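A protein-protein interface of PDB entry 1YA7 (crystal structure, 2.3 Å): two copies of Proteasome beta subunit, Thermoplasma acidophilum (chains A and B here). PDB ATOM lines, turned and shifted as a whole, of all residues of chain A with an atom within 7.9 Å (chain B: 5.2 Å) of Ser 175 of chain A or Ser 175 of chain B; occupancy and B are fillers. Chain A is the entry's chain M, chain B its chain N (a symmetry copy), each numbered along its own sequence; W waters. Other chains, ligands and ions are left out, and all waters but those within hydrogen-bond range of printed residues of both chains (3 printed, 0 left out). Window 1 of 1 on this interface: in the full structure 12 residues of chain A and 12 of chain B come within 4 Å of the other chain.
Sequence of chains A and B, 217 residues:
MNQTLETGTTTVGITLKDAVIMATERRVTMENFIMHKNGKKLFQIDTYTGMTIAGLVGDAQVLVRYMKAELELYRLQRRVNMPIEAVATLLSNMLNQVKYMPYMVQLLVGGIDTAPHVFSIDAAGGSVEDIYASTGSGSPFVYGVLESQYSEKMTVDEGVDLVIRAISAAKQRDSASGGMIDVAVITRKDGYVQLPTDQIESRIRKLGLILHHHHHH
OD1 of Asp 174 of chain B lies close to OD1 of Asn 32 of chain A (2.8 Å). The backbone carbonyl oxygen (O) of Asn 32 of chain A sits at hydrogen-bond distance from the backbone NH (N) of Ser 175 of chain B (2.7 Å). The backbone carbonyl oxygen (O) of Arg 173 of chain B is in hydrogen-bond range of the backbone NH (N) of Ile 34 of chain A (2.9 Å). The backbone NH (N) of Ile 34 of chain B sits at hydrogen-bond distance from the backbone carbonyl oxygen (O) of Arg 173 of chain A, 2.8 Å away. The side-chain carboxylate of Asp 174 of chain A sits close to the side-chain amide oxygen of Asn 32 of chain B. The backbone NH (N) of Ser 175 of chain A is in hydrogen-bond range of the backbone carbonyl oxygen (O) of Asn 32 of chain B, 2.9 Å away.
Hydrophobic or aromatic side chains of chain B that line the printed part of chain A: Phe 33 and Ile 34. Among the printed residues, 19 pairs touch across the chains.
Asn 32 of chain A touches Arg 173 of chain B, and with the chains exchanged Arg 173 of chain A touches Asn 32 of chain B. Asn 32 of chain A touches Ser 175 of chain B, and with the chains exchanged Ser 175 of chain A touches Asn 32 of chain B. Ile 34 of chain A touches Arg 173 of chain B, and with the chains exchanged Arg 173 of chain A touches Ile 34 of chain B. Asp 174 of chain A touches Ile 34 of chain B, but with the chains exchanged Ile 34 of chain A does not touch Asp 174 of chain B (4.01 Å). 11 positions are printed for both chains.
Among the printed residues, merely in contact across the chains: Ser 175 of chain A with Ser 175 of chain B (3.1 Å), Arg 173 of chain A with Asn 32 of chain B (3.5 Å), Arg 173 of chain A with Phe 33 of chain B (3.5 Å), Gln 172 of chain A with Ile 34 of chain B (3.6 Å), Phe 33 of chain A with Arg 173 of chain B (3.6 Å), Asn 32 of chain A with Arg 173 of chain B (3.6 Å), Ser 175 of chain A with Ile 34 of chain B (3.6 Å), Ile 34 of chain A with Ser 175 of chain B (3.7 Å), Ser 137 of chain A with Asn 32 of chain B (3.9 Å), Ser 175 of chain A with Arg 27 of chain B (3.9 Å), Asp 174 of chain A with Ile 34 of chain B (3.97 Å), Phe 141 of chain A with Phe 33 of chain B (3.97 Å) and Arg 27 of chain A with Ser 175 of chain B (3.98 Å).
Of the printed residues of chain B, Ser 137 of chain A touches Asn 32. Of the printed residues of chain B, Ser 175 of chain A touches Arg 27 (3.9 Å), Asn 32 (2.9 Å), Ile 34 (3.6 Å) and Ser 175 (3.1 Å). Of the printed residues of chain A, Asp 174 of chain B touches Asn 32. Printed residues of chain A within 4 Å of Ser 175 of chain B: Arg 27, Asn 32, Ile 34 and Ser 175. The nearest printed residue of chain B that does not touch Ser 175 of chain A is Glu 31 of chain B (4.3 Å). The nearest printed residue of chain B that does not touch Asp 174 of chain A is Phe 33 of chain B (5.2 Å).
Water W3 bridges OG of Ser 175 of chain B (2.7 Å) and O of Glu 31 of chain A (3.0 Å). Water W2 lies within hydrogen-bond range of the backbone carbonyl oxygen of Glu 31 of chain B (2.9 Å) and the side-chain hydroxyl of Ser 175 of chain A (2.9 Å). Water W1 lies within hydrogen-bond range of NH1 of Arg 27 of chain B (3.0 Å) and NH1 of Arg 27 of chain A (3.0 Å).
N of Arg 27 of chain A is in hydrogen-bond range of OE1 of Glu 25 of chain A, at 3.0 Å. The backbone carbonyl oxygen of Ser 175 of chain A is in hydrogen-bond range of the guanidinium group of Arg 27 of chain A. The guanidinium group (NH1) of Arg 27 of chain A sits at hydrogen-bond distance from the backbone carbonyl oxygen (O) of Ser 177 of chain A. OG of Ser 137 of chain A lies within hydrogen-bond range of OD2 of Asp 174 of chain A (2.7 Å). The backbone carbonyl oxygen (O) of Ser 177 of chain B lies within hydrogen-bond range of the guanidinium group (NH1) of Arg 27 of chain B, 3.4 Å away. The side-chain carboxylate of Asp 174 of chain B lies close to the backbone NH of Ala 176 of chain B (3.2 Å).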
ATOM      1  N   THR A   9      -1.618 -24.096  16.709  1.00  0.00           N
ATOM      2  CA  THR A   9      -2.142 -25.272  17.487  1.00  0.00           C
ATOM      3  C   THR A   9      -3.225 -25.932  16.660  1.00  0.00           C
ATOM      4  O   THR A   9      -3.945 -25.271  15.932  1.00  0.00           O
ATOM      5  CB  THR A   9      -2.683 -24.817  18.862  1.00  0.00           C
ATOM      6  OG1 THR A   9      -1.606 -24.734  19.814  1.00  0.00           O
ATOM      7  CG2 THR A   9      -3.652 -25.880  19.515  1.00  0.00           C
ATOM      8  N   GLU A  25      -1.698 -31.724  18.034  1.00  0.00           N
ATOM      9  CA  GLU A  25      -0.254 -31.752  17.786  1.00  0.00           C
ATOM     10  C   GLU A  25       0.479 -31.102  18.992  1.00  0.00           C
ATOM     11  O   GLU A  25      -0.119 -30.954  20.055  1.00  0.00           O
ATOM     12  CB  GLU A  25       0.116 -31.220  16.400  1.00  0.00           C
ATOM     13  CG  GLU A  25      -0.490 -29.884  16.019  1.00  0.00           C
ATOM     14  CD  GLU A  25      -0.147 -28.834  17.036  1.00  0.00           C
ATOM     15  OE1 GLU A  25       0.986 -28.326  16.972  1.00  0.00           O
ATOM     16  OE2 GLU A  25      -0.997 -28.580  17.913  1.00  0.00           O
ATOM     17  N   ARG A  27       3.201 -28.366  18.975  1.00  0.00           N
ATOM     18  CA  ARG A  27       4.111 -27.256  18.783  1.00  0.00           C
ATOM     19  C   ARG A  27       3.758 -26.069  19.668  1.00  0.00           C
ATOM     20  O   ARG A  27       2.624 -25.634  19.702  1.00  0.00           O
ATOM     21  CB  ARG A  27       4.149 -26.835  17.300  1.00  0.00           C
ATOM     22  CG  ARG A  27       5.094 -25.655  16.991  1.00  0.00           C
ATOM     23  CD  ARG A  27       5.243 -25.368  15.528  1.00  0.00           C
ATOM     24  NE  ARG A  27       6.005 -26.452  14.916  1.00  0.00           N
ATOM     25  CZ  ARG A  27       6.269 -26.552  13.630  1.00  0.00           C
ATOM     26  NH1 ARG A  27       5.870 -25.609  12.777  1.00  0.00           N
ATOM     27  NH2 ARG A  27       6.947 -27.598  13.195  1.00  0.00           N
ATOM     28  N   THR A  29       4.791 -22.151  19.950  1.00  0.00           N
ATOM     29  CA  THR A  29       5.474 -21.016  19.332  1.00  0.00           C
ATOM     30  C   THR A  29       5.308 -19.696  20.107  1.00  0.00           C
ATOM     31  O   THR A  29       4.352 -19.522  20.835  1.00  0.00           O
ATOM     32  CB  THR A  29       4.972 -20.777  17.880  1.00  0.00           C
ATOM     33  OG1 THR A  29       3.550 -20.736  17.878  1.00  0.00           O
ATOM     34  CG2 THR A  29       5.295 -21.935  16.965  1.00  0.00           C
ATOM     35  N   MET A  30       6.265 -18.781  19.934  1.00  0.00           N
ATOM     36  CA  MET A  30       6.119 -17.353  20.275  1.00  0.00           C
ATOM     37  C   MET A  30       6.374 -16.674  18.938  1.00  0.00           C
ATOM     38  O   MET A  30       7.519 -16.606  18.476  1.00  0.00           O
ATOM     39  CB  MET A  30       7.156 -16.934  21.340  1.00  0.00           C
ATOM     40  CG  MET A  30       7.550 -15.431  21.387  1.00  0.00           C
ATOM     41  SD  MET A  30       9.394 -15.180  21.382  1.00  0.00           S
ATOM     42  CE  MET A  30       9.803 -14.739  23.092  1.00  0.00           C
ATOM     43  N   GLU A  31       5.306 -16.228  18.284  1.00  0.00           N
ATOM     44  CA  GLU A  31       5.389 -15.832  16.891  1.00  0.00           C
ATOM     45  C   GLU A  31       5.853 -17.007  16.005  1.00  0.00           C
ATOM     46  O   GLU A  31       5.291 -18.107  16.085  1.00  0.00           O
ATOM     47  CB  GLU A  31       6.366 -14.684  16.731  1.00  0.00           C
ATOM     48  CG  GLU A  31       5.841 -13.579  15.862  1.00  0.00           C
ATOM     49  CD  GLU A  31       5.178 -12.541  16.723  1.00  0.00           C
ATOM     50  OE1 GLU A  31       4.089 -12.037  16.335  1.00  0.00           O
ATOM     51  OE2 GLU A  31       5.763 -12.274  17.805  1.00  0.00           O
ATOM     52  N   ASN A  32       6.879 -16.750  15.185  1.00  0.00           N
ATOM     53  CA  ASN A  32       7.517 -17.738  14.293  1.00  0.00           C
ATOM     54  C   ASN A  32       8.450 -18.699  15.035  1.00  0.00           C
ATOM     55  O   ASN A  32       8.821 -19.748  14.516  1.00  0.00           O
ATOM     56  CB  ASN A  32       8.316 -17.016  13.194  1.00  0.00           C
ATOM     57  CG  ASN A  32       9.525 -16.259  13.750  1.00  0.00           C
ATOM     58  OD1 ASN A  32      10.693 -16.630  13.489  1.00  0.00           O
ATOM     59  ND2 ASN A  32       9.255 -15.212  14.547  1.00  0.00           N
ATOM     60  N   PHE A  33       8.802 -18.328  16.260  1.00  0.00           N
ATOM     61  CA  PHE A  33       9.848 -18.996  17.045  1.00  0.00           C
ATOM     62  C   PHE A  33       9.316 -20.268  17.712  1.00  0.00           C
ATOM     63  O   PHE A  33       8.643 -20.214  18.737  1.00  0.00           O
ATOM     64  CB  PHE A  33      10.425 -17.985  18.070  1.00  0.00           C
ATOM     65  CG  PHE A  33      11.662 -18.460  18.812  1.00  0.00           C
ATOM     66  CD1 PHE A  33      12.122 -19.775  18.717  1.00  0.00           C
ATOM     67  CD2 PHE A  33      12.351 -17.568  19.662  1.00  0.00           C
ATOM     68  CE1 PHE A  33      13.258 -20.209  19.431  1.00  0.00           C
ATOM     69  CE2 PHE A  33      13.489 -17.977  20.396  1.00  0.00           C
ATOM     70  CZ  PHE A  33      13.944 -19.302  20.275  1.00  0.00           C
ATOM     71  N   ILE A  34       9.636 -21.428  17.134  1.00  0.00           N
ATOM     72  CA  ILE A  34       9.274 -22.716  17.738  1.00  0.00           C
ATOM     73  C   ILE A  34      10.107 -22.960  19.006  1.00  0.00           C
ATOM     74  O   ILE A  34      11.238 -23.457  18.957  1.00  0.00           O
ATOM     75  CB  ILE A  34       9.428 -23.881  16.721  1.00  0.00           C
ATOM     76  CG1 ILE A  34       8.622 -23.611  15.440  1.00  0.00           C
ATOM     77  CG2 ILE A  34       9.043 -25.220  17.384  1.00  0.00           C
ATOM     78  CD1 ILE A  34       9.089 -24.378  14.202  1.00  0.00           C
ATOM     79  N   SER A 137      -5.304 -22.523  15.538  1.00  0.00           N
ATOM     80  CA  SER A 137      -5.004 -21.970  14.222  1.00  0.00           C
ATOM     81  C   SER A 137      -5.115 -23.006  13.094  1.00  0.00           C
ATOM     82  O   SER A 137      -5.539 -22.653  11.983  1.00  0.00           O
ATOM     83  CB  SER A 137      -3.610 -21.364  14.249  1.00  0.00           C
ATOM     84  OG  SER A 137      -2.675 -22.313  14.742  1.00  0.00           O
ATOM     85  N   GLY A 138      -4.805 -24.285  13.364  1.00  0.00           N
ATOM     86  CA  GLY A 138      -4.925 -25.328  12.314  1.00  0.00           C
ATOM     87  C   GLY A 138      -6.335 -25.819  12.064  1.00  0.00           C
ATOM     88  O   GLY A 138      -6.556 -26.659  11.189  1.00  0.00           O
ATOM     89  N   PHE A 141      -8.315 -26.209   8.479  1.00  0.00           N
ATOM     90  CA  PHE A 141      -7.781 -27.322   7.667  1.00  0.00           C
ATOM     91  C   PHE A 141      -8.392 -28.642   8.118  1.00  0.00           C
ATOM     92  O   PHE A 141      -8.753 -29.481   7.275  1.00  0.00           O
ATOM     93  CB  PHE A 141      -6.243 -27.388   7.734  1.00  0.00           C
ATOM     94  CG  PHE A 141      -5.576 -26.081   7.397  1.00  0.00           C
ATOM     95  CD1 PHE A 141      -5.590 -25.590   6.095  1.00  0.00           C
ATOM     96  CD2 PHE A 141      -5.016 -25.293   8.396  1.00  0.00           C
ATOM     97  CE1 PHE A 141      -5.031 -24.354   5.801  1.00  0.00           C
ATOM     98  CE2 PHE A 141      -4.438 -24.055   8.101  1.00  0.00           C
ATOM     99  CZ  PHE A 141      -4.450 -23.591   6.811  1.00  0.00           C
ATOM    100  N   ALA A 170      -3.429 -30.215   8.598  1.00  0.00           N
ATOM    101  CA  ALA A 170      -3.264 -28.922   9.317  1.00  0.00           C
ATOM    102  C   ALA A 170      -1.788 -28.595   9.524  1.00  0.00           C
ATOM    103  O   ALA A 170      -1.368 -27.465   9.279  1.00  0.00           O
ATOM    104  CB  ALA A 170      -4.031 -28.918  10.660  1.00  0.00           C
ATOM    105  N   LYS A 171      -0.993 -29.601   9.903  1.00  0.00           N
ATOM    106  CA  LYS A 171       0.456 -29.451  10.019  1.00  0.00           C
ATOM    107  C   LYS A 171       1.141 -29.052   8.702  1.00  0.00           C
ATOM    108  O   LYS A 171       2.132 -28.352   8.717  1.00  0.00           O
ATOM    109  CB  LYS A 171       1.077 -30.738  10.526  1.00  0.00           C
ATOM    110  CG  LYS A 171       1.023 -30.905  12.053  1.00  0.00           C
ATOM    111  CD  LYS A 171       1.354 -32.343  12.531  1.00  0.00           C
ATOM    112  CE  LYS A 171       2.610 -32.874  11.930  1.00  0.00           C
ATOM    113  NZ  LYS A 171       3.012 -34.185  12.565  1.00  0.00           N
ATOM    114  N   GLN A 172       0.624 -29.501   7.566  1.00  0.00           N
ATOM    115  CA  GLN A 172       1.213 -29.143   6.292  1.00  0.00           C
ATOM    116  C   GLN A 172       0.919 -27.672   5.913  1.00  0.00           C
ATOM    117  O   GLN A 172       1.598 -27.110   5.072  1.00  0.00           O
ATOM    118  CB  GLN A 172       0.697 -30.094   5.184  1.00  0.00           C
ATOM    119  CG  GLN A 172       1.262 -31.546   5.252  1.00  0.00           C
ATOM    120  CD  GLN A 172       2.767 -31.590   5.010  1.00  0.00           C
ATOM    121  OE1 GLN A 172       3.279 -30.975   4.077  1.00  0.00           O
ATOM    122  NE2 GLN A 172       3.475 -32.269   5.880  1.00  0.00           N
ATOM    123  N   ARG A 173      -0.108 -27.075   6.503  1.00  0.00           N
ATOM    124  CA  ARG A 173      -0.588 -25.759   6.073  1.00  0.00           C
ATOM    125  C   ARG A 173      -0.595 -24.651   7.148  1.00  0.00           C
ATOM    126  O   ARG A 173      -0.777 -23.460   6.838  1.00  0.00           O
ATOM    127  CB  ARG A 173      -1.989 -25.904   5.466  1.00  0.00           C
ATOM    128  CG  ARG A 173      -1.998 -26.675   4.166  1.00  0.00           C
ATOM    129  CD  ARG A 173      -1.271 -25.942   3.063  1.00  0.00           C
ATOM    130  NE  ARG A 173      -0.902 -26.822   1.960  1.00  0.00           N
ATOM    131  CZ  ARG A 173      -0.365 -26.408   0.831  1.00  0.00           C
ATOM    132  NH1 ARG A 173      -0.111 -25.123   0.650  1.00  0.00           N
ATOM    133  NH2 ARG A 173      -0.075 -27.287  -0.123  1.00  0.00           N
ATOM    134  N   ASP A 174      -0.433 -25.052   8.398  1.00  0.00           N
ATOM    135  CA  ASP A 174      -0.449 -24.151   9.525  1.00  0.00           C
ATOM    136  C   ASP A 174       0.924 -24.222  10.219  1.00  0.00           C
ATOM    137  O   ASP A 174       1.207 -25.145  10.965  1.00  0.00           O
ATOM    138  CB  ASP A 174      -1.592 -24.498  10.495  1.00  0.00           C
ATOM    139  CG  ASP A 174      -1.517 -23.708  11.775  1.00  0.00           C
ATOM    140  OD1 ASP A 174      -1.054 -22.532  11.706  1.00  0.00           O
ATOM    141  OD2 ASP A 174      -1.855 -24.170  12.901  1.00  0.00           O
ATOM    142  N   SER A 175       1.748 -23.202  10.009  1.00  0.00           N
ATOM    143  CA  SER A 175       3.069 -23.203  10.555  1.00  0.00           C
ATOM    144  C   SER A 175       3.091 -23.150  12.091  1.00  0.00           C
ATOM    145  O   SER A 175       4.086 -23.537  12.685  1.00  0.00           O
ATOM    146  CB  SER A 175       3.927 -22.102   9.905  1.00  0.00           C
ATOM    147  OG  SER A 175       3.359 -20.846  10.177  1.00  0.00           O
ATOM    148  N   ALA A 176       1.992 -22.734  12.733  1.00  0.00           N
ATOM    149  CA  ALA A 176       1.884 -22.793  14.209  1.00  0.00           C
ATOM    150  C   ALA A 176       1.460 -24.175  14.730  1.00  0.00           C
ATOM    151  O   ALA A 176       1.041 -24.324  15.902  1.00  0.00           O
ATOM    152  CB  ALA A 176       0.885 -21.736  14.719  1.00  0.00           C
ATOM    153  N   SER A 177       1.444 -25.151  13.836  1.00  0.00           N
ATOM    154  CA  SER A 177       1.089 -26.537  14.200  1.00  0.00           C
ATOM    155  C   SER A 177       2.231 -27.437  13.808  1.00  0.00           C
ATOM    156  O   SER A 177       2.826 -27.266  12.760  1.00  0.00           O
ATOM    157  CB  SER A 177      -0.196 -26.979  13.499  1.00  0.00           C
ATOM    158  OG  SER A 177      -1.323 -26.356  14.129  1.00  0.00           O
ATOM    159  N   GLY A 178       2.563 -28.388  14.666  1.00  0.00           N
ATOM    160  CA  GLY A 178       3.546 -29.345  14.301  1.00  0.00           C
ATOM    161  C   GLY A 178       3.856 -30.297  15.424  1.00  0.00           C
ATOM    162  O   GLY A 178       3.195 -30.305  16.475  1.00  0.00           O
ATOM    163  N   ARG B  27       9.746 -21.860   1.838  1.00  0.00           N
ATOM    164  CA  ARG B  27       8.422 -21.643   2.375  1.00  0.00           C
ATOM    165  C   ARG B  27       7.938 -20.198   2.176  1.00  0.00           C
ATOM    166  O   ARG B  27       8.662 -19.232   2.435  1.00  0.00           O
ATOM    167  CB  ARG B  27       8.372 -22.014   3.870  1.00  0.00           C
ATOM    168  CG  ARG B  27       6.972 -21.898   4.463  1.00  0.00           C
ATOM    169  CD  ARG B  27       6.835 -22.437   5.858  1.00  0.00           C
ATOM    170  NE  ARG B  27       6.961 -23.887   5.842  1.00  0.00           N
ATOM    171  CZ  ARG B  27       6.940 -24.640   6.914  1.00  0.00           C
ATOM    172  NH1 ARG B  27       6.818 -24.083   8.135  1.00  0.00           N
ATOM    173  NH2 ARG B  27       7.066 -25.952   6.776  1.00  0.00           N
ATOM    174  N   THR B  29       4.734 -17.914   3.405  1.00  0.00           N
ATOM    175  CA  THR B  29       3.569 -17.836   4.284  1.00  0.00           C
ATOM    176  C   THR B  29       2.836 -16.492   4.181  1.00  0.00           C
ATOM    177  O   THR B  29       3.441 -15.498   3.807  1.00  0.00           O
ATOM    178  CB  THR B  29       4.017 -17.959   5.747  1.00  0.00           C
ATOM    179  OG1 THR B  29       5.139 -17.097   5.943  1.00  0.00           O
ATOM    180  CG2 THR B  29       4.552 -19.357   6.080  1.00  0.00           C
ATOM    181  N   GLU B  31       1.134 -14.805   7.336  1.00  0.00           N
ATOM    182  CA  GLU B  31       1.036 -15.100   8.750  1.00  0.00           C
ATOM    183  C   GLU B  31       1.448 -16.562   8.985  1.00  0.00           C
ATOM    184  O   GLU B  31       2.564 -16.949   8.619  1.00  0.00           O
ATOM    185  CB  GLU B  31      -0.377 -14.822   9.253  1.00  0.00           C
ATOM    186  CG  GLU B  31      -0.417 -14.237  10.657  1.00  0.00           C
ATOM    187  CD  GLU B  31      -0.493 -12.717  10.643  1.00  0.00           C
ATOM    188  OE1 GLU B  31      -0.615 -12.121  11.753  1.00  0.00           O
ATOM    189  OE2 GLU B  31      -0.442 -12.130   9.525  1.00  0.00           O
ATOM    190  N   ASN B  32       0.554 -17.353   9.584  1.00  0.00           N
ATOM    191  CA  ASN B  32       0.790 -18.784   9.857  1.00  0.00           C
ATOM    192  C   ASN B  32       0.439 -19.696   8.678  1.00  0.00           C
ATOM    193  O   ASN B  32       0.800 -20.870   8.664  1.00  0.00           O
ATOM    194  CB  ASN B  32       0.008 -19.252  11.111  1.00  0.00           C
ATOM    195  CG  ASN B  32      -1.505 -19.147  10.935  1.00  0.00           C
ATOM    196  OD1 ASN B  32      -2.219 -20.166  10.795  1.00  0.00           O
ATOM    197  ND2 ASN B  32      -2.000 -17.915  10.918  1.00  0.00           N
ATOM    198  N   PHE B  33      -0.279 -19.145   7.703  1.00  0.00           N
ATOM    199  CA  PHE B  33      -0.846 -19.919   6.601  1.00  0.00           C
ATOM    200  C   PHE B  33       0.271 -20.205   5.576  1.00  0.00           C
ATOM    201  O   PHE B  33       0.714 -19.302   4.854  1.00  0.00           O
ATOM    202  CB  PHE B  33      -2.032 -19.141   6.014  1.00  0.00           C
ATOM    203  CG  PHE B  33      -2.892 -19.908   5.016  1.00  0.00           C
ATOM    204  CD1 PHE B  33      -2.436 -21.064   4.360  1.00  0.00           C
ATOM    205  CD2 PHE B  33      -4.180 -19.426   4.699  1.00  0.00           C
ATOM    206  CE1 PHE B  33      -3.236 -21.729   3.419  1.00  0.00           C
ATOM    207  CE2 PHE B  33      -4.996 -20.088   3.750  1.00  0.00           C
ATOM    208  CZ  PHE B  33      -4.522 -21.244   3.116  1.00  0.00           C
ATOM    209  N   ILE B  34       0.755 -21.460   5.550  1.00  0.00           N
ATOM    210  CA  ILE B  34       1.692 -21.903   4.519  1.00  0.00           C
ATOM    211  C   ILE B  34       0.986 -21.966   3.155  1.00  0.00           C
ATOM    212  O   ILE B  34       0.322 -22.934   2.829  1.00  0.00           O
ATOM    213  CB  ILE B  34       2.346 -23.280   4.901  1.00  0.00           C
ATOM    214  CG1 ILE B  34       3.013 -23.205   6.289  1.00  0.00           C
ATOM    215  CG2 ILE B  34       3.316 -23.728   3.818  1.00  0.00           C
ATOM    216  CD1 ILE B  34       3.234 -24.524   6.978  1.00  0.00           C
ATOM    217  N   ARG B 173      13.348 -24.418  13.930  1.00  0.00           N
ATOM    218  CA  ARG B 173      13.056 -23.465  14.993  1.00  0.00           C
ATOM    219  C   ARG B 173      12.346 -22.215  14.521  1.00  0.00           C
ATOM    220  O   ARG B 173      11.949 -21.378  15.334  1.00  0.00           O
ATOM    221  CB  ARG B 173      14.382 -23.026  15.625  1.00  0.00           C
ATOM    222  CG  ARG B 173      15.003 -24.042  16.562  1.00  0.00           C
ATOM    223  CD  ARG B 173      14.122 -24.401  17.760  1.00  0.00           C
ATOM    224  NE  ARG B 173      14.543 -25.672  18.349  1.00  0.00           N
ATOM    225  CZ  ARG B 173      14.011 -26.241  19.426  1.00  0.00           C
ATOM    226  NH1 ARG B 173      13.015 -25.660  20.095  1.00  0.00           N
ATOM    227  NH2 ARG B 173      14.507 -27.387  19.845  1.00  0.00           N
ATOM    228  N   ASP B 174      12.240 -22.061  13.204  1.00  0.00           N
ATOM    229  CA  ASP B 174      11.577 -20.918  12.608  1.00  0.00           C
ATOM    230  C   ASP B 174      10.415 -21.475  11.782  1.00  0.00           C
ATOM    231  O   ASP B 174      10.618 -22.109  10.770  1.00  0.00           O
ATOM    232  CB  ASP B 174      12.544 -20.096  11.725  1.00  0.00           C
ATOM    233  CG  ASP B 174      11.830 -18.992  10.958  1.00  0.00           C
ATOM    234  OD1 ASP B 174      10.769 -18.565  11.453  1.00  0.00           O
ATOM    235  OD2 ASP B 174      12.196 -18.512   9.853  1.00  0.00           O
ATOM    236  N   SER B 175       9.197 -21.238  12.238  1.00  0.00           N
ATOM    237  CA  SER B 175       8.045 -21.800  11.595  1.00  0.00           C
ATOM    238  C   SER B 175       7.774 -21.176  10.228  1.00  0.00           C
ATOM    239  O   SER B 175       7.008 -21.741   9.445  1.00  0.00           O
ATOM    240  CB  SER B 175       6.823 -21.750  12.527  1.00  0.00           C
ATOM    241  OG  SER B 175       6.516 -20.421  12.830  1.00  0.00           O
ATOM    242  N   ALA B 176       8.419 -20.042   9.919  1.00  0.00           N
ATOM    243  CA  ALA B 176       8.259 -19.380   8.625  1.00  0.00           C
ATOM    244  C   ALA B 176       9.289 -19.847   7.597  1.00  0.00           C
ATOM    245  O   ALA B 176       9.409 -19.294   6.514  1.00  0.00           O
ATOM    246  CB  ALA B 176       8.302 -17.848   8.792  1.00  0.00           C
ATOM    247  N   SER B 177      10.036 -20.875   7.960  1.00  0.00           N
ATOM    248  CA  SER B 177      11.069 -21.466   7.101  1.00  0.00           C
ATOM    249  C   SER B 177      10.726 -22.927   6.901  1.00  0.00           C
ATOM    250  O   SER B 177      10.213 -23.561   7.821  1.00  0.00           O
ATOM    251  CB  SER B 177      12.425 -21.367   7.786  1.00  0.00           C
ATOM    252  OG  SER B 177      12.808 -20.011   7.829  1.00  0.00           O
HETATM  253  O   HOH W   1       7.055 -26.259  10.127  1.00  0.00           O
HETATM  254  O   HOH W   2       4.817 -18.370   9.737  1.00  0.00           O
HETATM  255  O   HOH W   3       4.107 -19.897  13.989  1.00  0.00           O
